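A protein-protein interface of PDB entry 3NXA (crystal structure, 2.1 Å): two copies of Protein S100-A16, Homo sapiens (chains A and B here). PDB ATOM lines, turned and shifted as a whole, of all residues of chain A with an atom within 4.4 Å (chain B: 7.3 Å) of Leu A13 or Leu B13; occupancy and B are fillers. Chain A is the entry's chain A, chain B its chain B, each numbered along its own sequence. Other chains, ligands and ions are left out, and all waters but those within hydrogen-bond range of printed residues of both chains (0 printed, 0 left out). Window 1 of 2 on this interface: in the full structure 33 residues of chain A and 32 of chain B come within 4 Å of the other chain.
Of the printed residues of chain B, Leu A6 touches Leu B13 and Asn B16. Of the printed residues of chain B, Val A12 touches Glu B5 (3.5 Å), Leu B6 (3.8 Å) and Ala B9 (3.6 Å). Of chain B, only Leu B6 and Leu B13 come within 4 Å of Leu A13. Printed residues of chain A within 4 Å of Val B12: Ala A9 (3.9 Å). Of the printed residues of chain A, Thr B85 touches Val A10, Val A14 and Trp A78. The nearest residue of chain A that does not touch Leu B13 is Trp A78 (4.2 Å). The nearest printed residue of chain A that does not touch Ala B9 is Leu A13 (4.6 Å).
The indole nitrogen of Trp A78 is in hydrogen-bond range of the backbone carbonyl oxygen of Trp B78 (2.8 Å). The backbone NH (N) of Gly B82 sits close to the indole nitrogen (NE1) of Trp A78 (3.4 Å).
Leu A6 touches Leu B13, and with the chains exchanged Leu A13 touches Leu B6. Ala B9 touches its own counterpart, Ala A9. Leu A13 touches its own counterpart, Leu B13. Trp A78 touches its own counterpart, Trp B78. Of the 17 pairs that touch across the chains among the printed residues, 9 have their exchanged pair printed and touching as well.
Among the printed residues, merely in contact across the chains: Val A10 with Thr B85, Val A12 with Glu B5, Leu A6 with Asn B16, Val A12 with Ala B9, Asn A16 with Leu B6, Ala A9 with Ala B9, Leu A13 with Leu B6, Trp A78 with Ile B81, Leu A6 with Leu B13, Val A14 with Thr B85, Ala A9 with Leu B13, Trp A78 with Thr B85, Val A12 with Leu B6, Ala A9 with Val B12 and Leu A13 with Leu B13.
Hydrophobic or aromatic side chains of chain A within 4 Å of the printed part of chain B: Leu A6, Ala A9, Val A10, Val A12, Leu A13, Val A14 and Trp A78. Printed residues of chain B that touch a printed residue of chain A: Glu B5, Leu B6, Ala B9, Val B12, Leu B13, Asn B16, Trp B78, Ile B81, Gly B82 and Thr B85.
The side-chain amide nitrogen (ND2) of Asn A16 is in hydrogen-bond range of the side-chain hydroxyl (OH) of Tyr A77 (2.9 Å). O of Leu A13 sits at hydrogen-bond distance from OH of Tyr A77, 2.5 Å away. The side-chain amide nitrogen (ND2) of Asn B16 lies within hydrogen-bond range of the side-chain hydroxyl (OH) of Tyr B77 (2.9 Å). OH of Tyr B77 is in hydrogen-bond range of O of Leu B13. ND2 of Asn B16 is in hydrogen-bond range of SD of Met B39 (3.3 Å). The side-chain amino group of Lys B8 lies within salt-bridge range of the side-chain carboxylate of Glu B5 (3.7 Å).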
ATOM      1  N   LEU A   6     -12.624 -12.433   5.314  1.00  0.00           N
ATOM      2  CA  LEU A   6     -11.842 -12.979   6.461  1.00  0.00           C
ATOM      3  C   LEU A   6     -10.444 -12.521   6.431  1.00  0.00           C
ATOM      4  O   LEU A   6      -9.850 -12.146   7.483  1.00  0.00           O
ATOM      5  CB  LEU A   6     -11.794 -14.566   6.346  1.00  0.00           C
ATOM      6  CG  LEU A   6     -10.961 -15.275   7.489  1.00  0.00           C
ATOM      7  CD1 LEU A   6     -11.740 -14.886   8.786  1.00  0.00           C
ATOM      8  CD2 LEU A   6     -11.035 -16.830   7.300  1.00  0.00           C
ATOM      9  N   ALA A   9     -10.067  -9.207   7.713  1.00  0.00           N
ATOM     10  CA  ALA A   9     -10.268  -9.016   9.170  1.00  0.00           C
ATOM     11  C   ALA A   9      -9.065  -9.446   9.920  1.00  0.00           C
ATOM     12  O   ALA A   9      -8.861  -9.041  11.081  1.00  0.00           O
ATOM     13  CB  ALA A   9     -11.449  -9.968   9.630  1.00  0.00           C
ATOM     14  N   VAL A  10      -8.392 -10.510   9.464  1.00  0.00           N
ATOM     15  CA  VAL A  10      -7.048 -10.923  10.092  1.00  0.00           C
ATOM     16  C   VAL A  10      -6.119  -9.847   9.981  1.00  0.00           C
ATOM     17  O   VAL A  10      -5.437  -9.451  10.907  1.00  0.00           O
ATOM     18  CB  VAL A  10      -6.472 -12.401   9.495  1.00  0.00           C
ATOM     19  CG1 VAL A  10      -5.078 -12.703  10.185  1.00  0.00           C
ATOM     20  CG2 VAL A  10      -7.514 -13.414   9.680  1.00  0.00           C
ATOM     21  N   ILE A  11      -6.054  -9.241   8.791  1.00  0.00           N
ATOM     22  CA  ILE A  11      -5.254  -8.014   8.771  1.00  0.00           C
ATOM     23  C   ILE A  11      -5.546  -6.921   9.767  1.00  0.00           C
ATOM     24  O   ILE A  11      -4.546  -6.342  10.424  1.00  0.00           O
ATOM     25  CB  ILE A  11      -5.154  -7.336   7.158  1.00  0.00           C
ATOM     26  CG1 ILE A  11      -4.299  -8.226   6.427  1.00  0.00           C
ATOM     27  CG2 ILE A  11      -4.654  -5.957   7.225  1.00  0.00           C
ATOM     28  CD1 ILE A  11      -4.526  -8.123   4.986  1.00  0.00           C
ATOM     29  N   VAL A  12      -6.857  -6.581   9.904  1.00  0.00           N
ATOM     30  CA  VAL A  12      -7.171  -5.563  10.989  1.00  0.00           C
ATOM     31  C   VAL A  12      -6.678  -6.191  12.387  1.00  0.00           C
ATOM     32  O   VAL A  12      -6.082  -5.508  13.295  1.00  0.00           O
ATOM     33  CB  VAL A  12      -8.769  -5.455  11.094  1.00  0.00           C
ATOM     34  CG1 VAL A  12      -9.288  -4.906  12.453  1.00  0.00           C
ATOM     35  CG2 VAL A  12      -9.319  -4.613  10.105  1.00  0.00           C
ATOM     36  N   LEU A  13      -7.038  -7.397  12.666  1.00  0.00           N
ATOM     37  CA  LEU A  13      -6.504  -7.903  13.973  1.00  0.00           C
ATOM     38  C   LEU A  13      -5.011  -7.721  14.207  1.00  0.00           C
ATOM     39  O   LEU A  13      -4.591  -7.510  15.379  1.00  0.00           O
ATOM     40  CB  LEU A  13      -6.954  -9.249  14.216  1.00  0.00           C
ATOM     41  CG  LEU A  13      -8.427  -9.427  14.765  1.00  0.00           C
ATOM     42  CD1 LEU A  13      -8.903 -10.627  14.264  1.00  0.00           C
ATOM     43  CD2 LEU A  13      -8.386  -9.408  15.908  1.00  0.00           C
ATOM     44  N   VAL A  14      -4.216  -7.792  13.120  1.00  0.00           N
ATOM     45  CA  VAL A  14      -2.789  -7.866  13.127  1.00  0.00           C
ATOM     46  C   VAL A  14      -2.338  -6.366  13.144  1.00  0.00           C
ATOM     47  O   VAL A  14      -1.546  -5.975  14.105  1.00  0.00           O
ATOM     48  CB  VAL A  14      -2.065  -8.695  11.928  1.00  0.00           C
ATOM     49  CG1 VAL A  14      -0.671  -8.113  11.443  1.00  0.00           C
ATOM     50  CG2 VAL A  14      -2.031 -10.104  12.020  1.00  0.00           C
ATOM     51  N   GLU A  15      -2.976  -5.553  12.267  1.00  0.00           N
ATOM     52  CA  GLU A  15      -2.619  -4.045  12.425  1.00  0.00           C
ATOM     53  C   GLU A  15      -2.958  -3.389  13.847  1.00  0.00           C
ATOM     54  O   GLU A  15      -2.376  -2.529  14.385  1.00  0.00           O
ATOM     55  CB  GLU A  15      -3.316  -3.179  11.194  1.00  0.00           C
ATOM     56  CG  GLU A  15      -2.492  -3.838   9.994  1.00  0.00           C
ATOM     57  CD  GLU A  15      -1.010  -3.267  10.047  1.00  0.00           C
ATOM     58  OE1 GLU A  15      -0.680  -2.046   9.782  1.00  0.00           O
ATOM     59  OE2 GLU A  15      -0.070  -3.997  10.271  1.00  0.00           O
ATOM     60  N   ASN A  16      -3.900  -3.901  14.501  1.00  0.00           N
ATOM     61  CA  ASN A  16      -4.400  -3.449  15.696  1.00  0.00           C
ATOM     62  C   ASN A  16      -3.573  -3.850  16.831  1.00  0.00           C
ATOM     63  O   ASN A  16      -3.341  -2.933  17.708  1.00  0.00           O
ATOM     64  CB  ASN A  16      -5.760  -3.869  15.830  1.00  0.00           C
ATOM     65  CG  ASN A  16      -6.271  -3.611  17.222  1.00  0.00           C
ATOM     66  OD1 ASN A  16      -6.751  -2.391  17.536  1.00  0.00           O
ATOM     67  ND2 ASN A  16      -6.207  -4.703  18.118  1.00  0.00           N
ATOM     68  N   PHE A  17      -2.867  -4.947  16.777  1.00  0.00           N
ATOM     69  CA  PHE A  17      -1.939  -5.243  17.706  1.00  0.00           C
ATOM     70  C   PHE A  17      -0.766  -4.312  17.506  1.00  0.00           C
ATOM     71  O   PHE A  17      -0.083  -3.883  18.481  1.00  0.00           O
ATOM     72  CB  PHE A  17      -1.286  -6.672  17.392  1.00  0.00           C
ATOM     73  CG  PHE A  17       0.014  -7.131  18.494  1.00  0.00           C
ATOM     74  CD1 PHE A  17      -0.233  -7.642  19.740  1.00  0.00           C
ATOM     75  CD2 PHE A  17       1.291  -7.217  18.061  1.00  0.00           C
ATOM     76  CE1 PHE A  17       0.814  -8.050  20.595  1.00  0.00           C
ATOM     77  CE2 PHE A  17       2.506  -7.619  18.816  1.00  0.00           C
ATOM     78  CZ  PHE A  17       2.212  -8.003  20.250  1.00  0.00           C
ATOM     79  N   TYR A  77      -1.882 -12.193  22.673  1.00  0.00           N
ATOM     80  CA  TYR A  77      -2.863 -11.053  22.536  1.00  0.00           C
ATOM     81  C   TYR A  77      -4.037 -11.850  21.733  1.00  0.00           C
ATOM     82  O   TYR A  77      -5.266 -11.673  21.921  1.00  0.00           O
ATOM     83  CB  TYR A  77      -2.236 -10.048  21.532  1.00  0.00           C
ATOM     84  CG  TYR A  77      -3.244  -9.452  20.369  1.00  0.00           C
ATOM     85  CD1 TYR A  77      -4.069  -8.409  20.721  1.00  0.00           C
ATOM     86  CD2 TYR A  77      -3.172  -9.832  19.097  1.00  0.00           C
ATOM     87  CE1 TYR A  77      -4.885  -7.712  19.734  1.00  0.00           C
ATOM     88  CE2 TYR A  77      -4.054  -9.122  17.958  1.00  0.00           C
ATOM     89  CZ  TYR A  77      -4.782  -8.085  18.372  1.00  0.00           C
ATOM     90  OH  TYR A  77      -5.645  -7.503  17.620  1.00  0.00           O
ATOM     91  N   TRP A  78      -3.688 -12.704  20.844  1.00  0.00           N
ATOM     92  CA  TRP A  78      -4.656 -13.361  20.001  1.00  0.00           C
ATOM     93  C   TRP A  78      -5.532 -14.259  21.001  1.00  0.00           C
ATOM     94  O   TRP A  78      -6.799 -14.347  20.918  1.00  0.00           O
ATOM     95  CB  TRP A  78      -3.801 -14.287  19.043  1.00  0.00           C
ATOM     96  CG  TRP A  78      -4.845 -14.922  18.062  1.00  0.00           C
ATOM     97  CD1 TRP A  78      -5.481 -16.143  18.201  1.00  0.00           C
ATOM     98  CD2 TRP A  78      -5.407 -14.268  16.830  1.00  0.00           C
ATOM     99  NE1 TRP A  78      -6.456 -16.273  17.219  1.00  0.00           N
ATOM    100  CE2 TRP A  78      -6.320 -15.223  16.278  1.00  0.00           C
ATOM    101  CE3 TRP A  78      -5.110 -13.048  16.136  1.00  0.00           C
ATOM    102  CZ2 TRP A  78      -7.115 -14.968  15.121  1.00  0.00           C
ATOM    103  CZ3 TRP A  78      -5.650 -12.951  14.639  1.00  0.00           C
ATOM    104  CH2 TRP A  78      -6.689 -13.826  14.293  1.00  0.00           C
ATOM    105  N   GLU B   5     -13.273  -0.643  14.032  1.00  0.00           N
ATOM    106  CA  GLU B   5     -12.836  -1.600  12.971  1.00  0.00           C
ATOM    107  C   GLU B   5     -12.371  -2.919  13.552  1.00  0.00           C
ATOM    108  O   GLU B   5     -12.630  -3.834  12.885  1.00  0.00           O
ATOM    109  CB  GLU B   5     -11.766  -1.096  12.025  1.00  0.00           C
ATOM    110  CG  GLU B   5     -11.989   0.213  11.653  1.00  0.00           C
ATOM    111  CD  GLU B   5     -13.106   0.481  10.471  1.00  0.00           C
ATOM    112  OE1 GLU B   5     -13.723  -0.461   9.952  1.00  0.00           O
ATOM    113  OE2 GLU B   5     -13.377   1.678   9.990  1.00  0.00           O
ATOM    114  N   LEU B   6     -11.845  -3.007  14.826  1.00  0.00           N
ATOM    115  CA  LEU B   6     -11.417  -4.207  15.528  1.00  0.00           C
ATOM    116  C   LEU B   6     -12.698  -5.005  15.910  1.00  0.00           C
ATOM    117  O   LEU B   6     -12.816  -6.214  15.708  1.00  0.00           O
ATOM    118  CB  LEU B   6     -10.756  -3.814  16.826  1.00  0.00           C
ATOM    119  CG  LEU B   6     -10.591  -5.152  17.645  1.00  0.00           C
ATOM    120  CD1 LEU B   6      -9.699  -6.154  17.019  1.00  0.00           C
ATOM    121  CD2 LEU B   6      -9.741  -4.912  18.909  1.00  0.00           C
ATOM    122  N   GLU B   7     -13.784  -4.337  16.420  1.00  0.00           N
ATOM    123  CA  GLU B   7     -15.034  -5.027  16.560  1.00  0.00           C
ATOM    124  C   GLU B   7     -15.549  -5.574  15.326  1.00  0.00           C
ATOM    125  O   GLU B   7     -16.125  -6.718  15.354  1.00  0.00           O
ATOM    126  CB  GLU B   7     -16.147  -4.065  17.253  1.00  0.00           C
ATOM    127  CG  GLU B   7     -15.948  -4.147  18.631  1.00  0.00           C
ATOM    128  CD  GLU B   7     -16.501  -2.855  19.376  1.00  0.00           C
ATOM    129  OE1 GLU B   7     -16.939  -1.943  18.625  1.00  0.00           O
ATOM    130  OE2 GLU B   7     -16.306  -2.753  20.662  1.00  0.00           O
ATOM    131  N   LYS B   8     -15.513  -4.835  14.226  1.00  0.00           N
ATOM    132  CA  LYS B   8     -16.288  -5.401  13.088  1.00  0.00           C
ATOM    133  C   LYS B   8     -15.447  -6.652  12.525  1.00  0.00           C
ATOM    134  O   LYS B   8     -15.941  -7.623  11.871  1.00  0.00           O
ATOM    135  CB  LYS B   8     -16.119  -4.469  11.987  1.00  0.00           C
ATOM    136  CG  LYS B   8     -17.049  -3.471  12.151  1.00  0.00           C
ATOM    137  CD  LYS B   8     -17.269  -2.858  10.691  1.00  0.00           C
ATOM    138  CE  LYS B   8     -17.211  -1.400  10.720  1.00  0.00           C
ATOM    139  NZ  LYS B   8     -15.823  -1.132   9.955  1.00  0.00           N
ATOM    140  N   ALA B   9     -14.107  -6.633  12.796  1.00  0.00           N
ATOM    141  CA  ALA B   9     -13.311  -7.845  12.368  1.00  0.00           C
ATOM    142  C   ALA B   9     -13.540  -9.005  13.355  1.00  0.00           C
ATOM    143  O   ALA B   9     -13.606 -10.088  12.890  1.00  0.00           O
ATOM    144  CB  ALA B   9     -11.831  -7.397  12.476  1.00  0.00           C
ATOM    145  N   VAL B  10     -13.765  -8.816  14.668  1.00  0.00           N
ATOM    146  CA  VAL B  10     -14.104  -9.943  15.488  1.00  0.00           C
ATOM    147  C   VAL B  10     -15.321 -10.486  14.951  1.00  0.00           C
ATOM    148  O   VAL B  10     -15.475 -11.673  14.743  1.00  0.00           O
ATOM    149  CB  VAL B  10     -14.232  -9.413  16.748  1.00  0.00           C
ATOM    150  CG1 VAL B  10     -14.788 -10.626  17.618  1.00  0.00           C
ATOM    151  CG2 VAL B  10     -12.810  -9.265  17.153  1.00  0.00           C
ATOM    152  N   ILE B  11     -16.344  -9.683  14.756  1.00  0.00           N
ATOM    153  CA  ILE B  11     -17.597 -10.162  14.142  1.00  0.00           C
ATOM    154  C   ILE B  11     -17.244 -10.862  12.936  1.00  0.00           C
ATOM    155  O   ILE B  11     -17.971 -11.764  12.507  1.00  0.00           O
ATOM    156  CB  ILE B  11     -18.663  -8.835  13.643  1.00  0.00           C
ATOM    157  CG1 ILE B  11     -19.277  -8.132  14.841  1.00  0.00           C
ATOM    158  CG2 ILE B  11     -19.720  -9.186  12.648  1.00  0.00           C
ATOM    159  CD1 ILE B  11     -18.510  -8.743  16.216  1.00  0.00           C
ATOM    160  N   VAL B  12     -16.395 -10.396  12.136  1.00  0.00           N
ATOM    161  CA  VAL B  12     -16.284 -11.190  10.691  1.00  0.00           C
ATOM    162  C   VAL B  12     -15.623 -12.583  10.998  1.00  0.00           C
ATOM    163  O   VAL B  12     -16.147 -13.574  10.526  1.00  0.00           O
ATOM    164  CB  VAL B  12     -15.516 -10.455   9.762  1.00  0.00           C
ATOM    165  CG1 VAL B  12     -14.980 -11.353   8.562  1.00  0.00           C
ATOM    166  CG2 VAL B  12     -16.459  -9.437   9.166  1.00  0.00           C
ATOM    167  N   LEU B  13     -14.919 -12.701  12.178  1.00  0.00           N
ATOM    168  CA  LEU B  13     -14.323 -14.119  12.470  1.00  0.00           C
ATOM    169  C   LEU B  13     -15.443 -15.042  12.945  1.00  0.00           C
ATOM    170  O   LEU B  13     -15.574 -16.311  12.549  1.00  0.00           O
ATOM    171  CB  LEU B  13     -13.155 -14.008  13.410  1.00  0.00           C
ATOM    172  CG  LEU B  13     -12.027 -14.000  12.402  1.00  0.00           C
ATOM    173  CD1 LEU B  13     -11.675 -12.637  12.298  1.00  0.00           C
ATOM    174  CD2 LEU B  13     -10.741 -14.491  13.041  1.00  0.00           C
ATOM    175  N   VAL B  14     -16.444 -14.445  13.578  1.00  0.00           N
ATOM    176  CA  VAL B  14     -17.675 -15.188  14.049  1.00  0.00           C
ATOM    177  C   VAL B  14     -18.586 -15.438  12.816  1.00  0.00           C
ATOM    178  O   VAL B  14     -19.029 -16.587  12.559  1.00  0.00           O
ATOM    179  CB  VAL B  14     -18.297 -14.328  15.157  1.00  0.00           C
ATOM    180  CG1 VAL B  14     -19.732 -14.837  15.705  1.00  0.00           C
ATOM    181  CG2 VAL B  14     -17.443 -14.235  16.508  1.00  0.00           C
ATOM    182  N   GLU B  15     -18.845 -14.473  11.968  1.00  0.00           N
ATOM    183  CA  GLU B  15     -19.807 -14.930  10.883  1.00  0.00           C
ATOM    184  C   GLU B  15     -19.237 -15.892  10.021  1.00  0.00           C
ATOM    185  O   GLU B  15     -19.902 -16.920   9.450  1.00  0.00           O
ATOM    186  CB  GLU B  15     -20.271 -13.625  10.158  1.00  0.00           C
ATOM    187  CG  GLU B  15     -21.133 -12.788  11.139  1.00  0.00           C
ATOM    188  CD  GLU B  15     -22.435 -13.542  11.178  1.00  0.00           C
ATOM    189  OE1 GLU B  15     -23.094 -13.710  10.119  1.00  0.00           O
ATOM    190  OE2 GLU B  15     -22.810 -14.120  12.218  1.00  0.00           O
ATOM    191  N   ASN B  16     -17.929 -15.748   9.749  1.00  0.00           N
ATOM    192  CA  ASN B  16     -17.196 -16.764   8.951  1.00  0.00           C
ATOM    193  C   ASN B  16     -17.215 -18.240   9.566  1.00  0.00           C
ATOM    194  O   ASN B  16     -17.400 -19.231   8.864  1.00  0.00           O
ATOM    195  CB  ASN B  16     -15.712 -16.277   8.908  1.00  0.00           C
ATOM    196  CG  ASN B  16     -14.872 -17.369   8.146  1.00  0.00           C
ATOM    197  OD1 ASN B  16     -15.094 -17.625   6.906  1.00  0.00           O
ATOM    198  ND2 ASN B  16     -13.944 -18.036   8.922  1.00  0.00           N
ATOM    199  N   PHE B  17     -17.079 -18.394  10.878  1.00  0.00           N
ATOM    200  CA  PHE B  17     -17.069 -19.764  11.397  1.00  0.00           C
ATOM    201  C   PHE B  17     -18.506 -20.308  11.260  1.00  0.00           C
ATOM    202  O   PHE B  17     -18.760 -21.522  10.697  1.00  0.00           O
ATOM    203  CB  PHE B  17     -16.774 -19.504  12.887  1.00  0.00           C
ATOM    204  CG  PHE B  17     -16.980 -20.777  13.826  1.00  0.00           C
ATOM    205  CD1 PHE B  17     -16.017 -21.740  13.912  1.00  0.00           C
ATOM    206  CD2 PHE B  17     -18.331 -21.111  14.235  1.00  0.00           C
ATOM    207  CE1 PHE B  17     -16.193 -22.911  14.799  1.00  0.00           C
ATOM    208  CE2 PHE B  17     -18.548 -22.313  15.097  1.00  0.00           C
ATOM    209  CZ  PHE B  17     -17.393 -23.082  15.391  1.00  0.00           C
ATOM    210  N   TYR B  18     -19.473 -19.568  11.603  1.00  0.00           N
ATOM    211  CA  TYR B  18     -20.915 -20.108  11.512  1.00  0.00           C
ATOM    212  C   TYR B  18     -21.260 -20.158  10.031  1.00  0.00           C
ATOM    213  O   TYR B  18     -22.087 -21.017   9.688  1.00  0.00           O
ATOM    214  CB  TYR B  18     -22.082 -19.293  12.269  1.00  0.00           C
ATOM    215  CG  TYR B  18     -22.022 -19.452  13.720  1.00  0.00           C
ATOM    216  CD1 TYR B  18     -22.676 -20.489  14.318  1.00  0.00           C
ATOM    217  CD2 TYR B  18     -21.379 -18.517  14.501  1.00  0.00           C
ATOM    218  CE1 TYR B  18     -22.562 -20.672  15.630  1.00  0.00           C
ATOM    219  CE2 TYR B  18     -21.314 -18.672  15.842  1.00  0.00           C
ATOM    220  CZ  TYR B  18     -21.907 -19.820  16.405  1.00  0.00           C
ATOM    221  OH  TYR B  18     -21.955 -20.071  17.668  1.00  0.00           O
ATOM    222  N   LYS B  19     -20.631 -19.313   9.143  1.00  0.00           N
ATOM    223  CA  LYS B  19     -21.014 -19.686   7.725  1.00  0.00           C
ATOM    224  C   LYS B  19     -20.609 -21.192   7.369  1.00  0.00           C
ATOM    225  O   LYS B  19     -21.125 -21.831   6.388  1.00  0.00           O
ATOM    226  CB  LYS B  19     -20.063 -18.925   6.830  1.00  0.00           C
ATOM    227  CG  LYS B  19     -20.390 -18.676   5.252  1.00  0.00           C
ATOM    228  CD  LYS B  19     -19.161 -17.739   4.701  1.00  0.00           C
ATOM    229  CE  LYS B  19     -18.819 -18.172   3.143  1.00  0.00           C
ATOM    230  NZ  LYS B  19     -18.323 -16.992   2.370  1.00  0.00           N
ATOM    231  N   MET B  39     -12.903 -23.865   4.199  1.00  0.00           N
ATOM    232  CA  MET B  39     -12.740 -22.486   4.586  1.00  0.00           C
ATOM    233  C   MET B  39     -11.387 -22.028   4.340  1.00  0.00           C
ATOM    234  O   MET B  39     -11.059 -20.741   4.031  1.00  0.00           O
ATOM    235  CB  MET B  39     -13.383 -22.055   6.065  1.00  0.00           C
ATOM    236  CG  MET B  39     -12.901 -20.760   6.557  1.00  0.00           C
ATOM    237  SD  MET B  39     -12.661 -21.075   8.393  1.00  0.00           S
ATOM    238  CE  MET B  39     -11.108 -21.620   8.150  1.00  0.00           C
ATOM    239  N   PHE B  74     -15.937 -23.249  18.321  1.00  0.00           N
ATOM    240  CA  PHE B  74     -15.515 -21.967  18.092  1.00  0.00           C
ATOM    241  C   PHE B  74     -14.114 -21.767  18.712  1.00  0.00           C
ATOM    242  O   PHE B  74     -13.345 -21.102  18.146  1.00  0.00           O
ATOM    243  CB  PHE B  74     -16.613 -20.965  18.717  1.00  0.00           C
ATOM    244  CG  PHE B  74     -16.138 -19.587  18.401  1.00  0.00           C
ATOM    245  CD1 PHE B  74     -16.368 -19.037  17.062  1.00  0.00           C
ATOM    246  CD2 PHE B  74     -15.375 -18.849  19.276  1.00  0.00           C
ATOM    247  CE1 PHE B  74     -16.042 -17.787  16.773  1.00  0.00           C
ATOM    248  CE2 PHE B  74     -14.734 -17.590  18.764  1.00  0.00           C
ATOM    249  CZ  PHE B  74     -15.130 -17.094  17.316  1.00  0.00           C
ATOM    250  N   TYR B  77     -11.376 -23.329  16.611  1.00  0.00           N
ATOM    251  CA  TYR B  77     -11.172 -22.563  15.365  1.00  0.00           C
ATOM    252  C   TYR B  77     -10.498 -21.196  15.509  1.00  0.00           C
ATOM    253  O   TYR B  77      -9.613 -20.839  14.732  1.00  0.00           O
ATOM    254  CB  TYR B  77     -12.559 -22.301  14.779  1.00  0.00           C
ATOM    255  CG  TYR B  77     -12.695 -20.913  14.051  1.00  0.00           C
ATOM    256  CD1 TYR B  77     -12.654 -20.871  12.736  1.00  0.00           C
ATOM    257  CD2 TYR B  77     -13.238 -19.792  14.686  1.00  0.00           C
ATOM    258  CE1 TYR B  77     -12.968 -19.681  11.970  1.00  0.00           C
ATOM    259  CE2 TYR B  77     -13.382 -18.559  14.003  1.00  0.00           C
ATOM    260  CZ  TYR B  77     -13.314 -18.626  12.578  1.00  0.00           C
ATOM    261  OH  TYR B  77     -13.457 -17.573  11.746  1.00  0.00           O
ATOM    262  N   TRP B  78     -10.805 -20.482  16.574  1.00  0.00           N
ATOM    263  CA  TRP B  78     -10.124 -19.279  16.863  1.00  0.00           C
ATOM    264  C   TRP B  78      -8.658 -19.546  17.030  1.00  0.00           C
ATOM    265  O   TRP B  78      -7.780 -18.641  16.748  1.00  0.00           O
ATOM    266  CB  TRP B  78     -10.651 -18.666  18.250  1.00  0.00           C
ATOM    267  CG  TRP B  78     -10.053 -17.279  18.518  1.00  0.00           C
ATOM    268  CD1 TRP B  78      -8.802 -16.950  19.302  1.00  0.00           C
ATOM    269  CD2 TRP B  78     -10.522 -15.956  17.954  1.00  0.00           C
ATOM    270  NE1 TRP B  78      -8.670 -15.549  19.262  1.00  0.00           N
ATOM    271  CE2 TRP B  78      -9.726 -14.971  18.497  1.00  0.00           C
ATOM    272  CE3 TRP B  78     -11.555 -15.596  17.020  1.00  0.00           C
ATOM    273  CZ2 TRP B  78      -9.878 -13.625  18.091  1.00  0.00           C
ATOM    274  CZ3 TRP B  78     -11.845 -14.309  16.853  1.00  0.00           C
ATOM    275  CH2 TRP B  78     -11.056 -13.315  17.314  1.00  0.00           C
ATOM    276  N   ILE B  81      -7.206 -20.322  13.604  1.00  0.00           N
ATOM    277  CA  ILE B  81      -6.870 -19.154  12.846  1.00  0.00           C
ATOM    278  C   ILE B  81      -5.575 -18.381  13.437  1.00  0.00           C
ATOM    279  O   ILE B  81      -4.745 -17.919  12.769  1.00  0.00           O
ATOM    280  CB  ILE B  81      -7.992 -18.164  12.928  1.00  0.00           C
ATOM    281  CG1 ILE B  81      -9.249 -18.902  12.052  1.00  0.00           C
ATOM    282  CG2 ILE B  81      -7.477 -16.970  12.007  1.00  0.00           C
ATOM    283  CD1 ILE B  81      -8.723 -19.322  10.639  1.00  0.00           C
ATOM    284  N   GLY B  82      -5.457 -18.339  14.739  1.00  0.00           N
ATOM    285  CA  GLY B  82      -4.276 -17.856  15.205  1.00  0.00           C
ATOM    286  C   GLY B  82      -3.071 -18.569  15.071  1.00  0.00           C
ATOM    287  O   GLY B  82      -1.922 -17.971  15.085  1.00  0.00           O
ATOM    288  N   THR B  85      -1.948 -17.400  11.630  1.00  0.00           N
ATOM    289  CA  THR B  85      -1.693 -15.968  11.674  1.00  0.00           C
ATOM    290  C   THR B  85      -0.497 -15.622  12.530  1.00  0.00           C
ATOM    291  O   THR B  85       0.337 -14.949  12.038  1.00  0.00           O
ATOM    292  CB  THR B  85      -2.997 -15.117  12.385  1.00  0.00           C
ATOM    293  OG1 THR B  85      -4.211 -15.307  11.532  1.00  0.00           O
ATOM    294  CG2 THR B  85      -2.723 -13.787  12.380  1.00  0.00           C
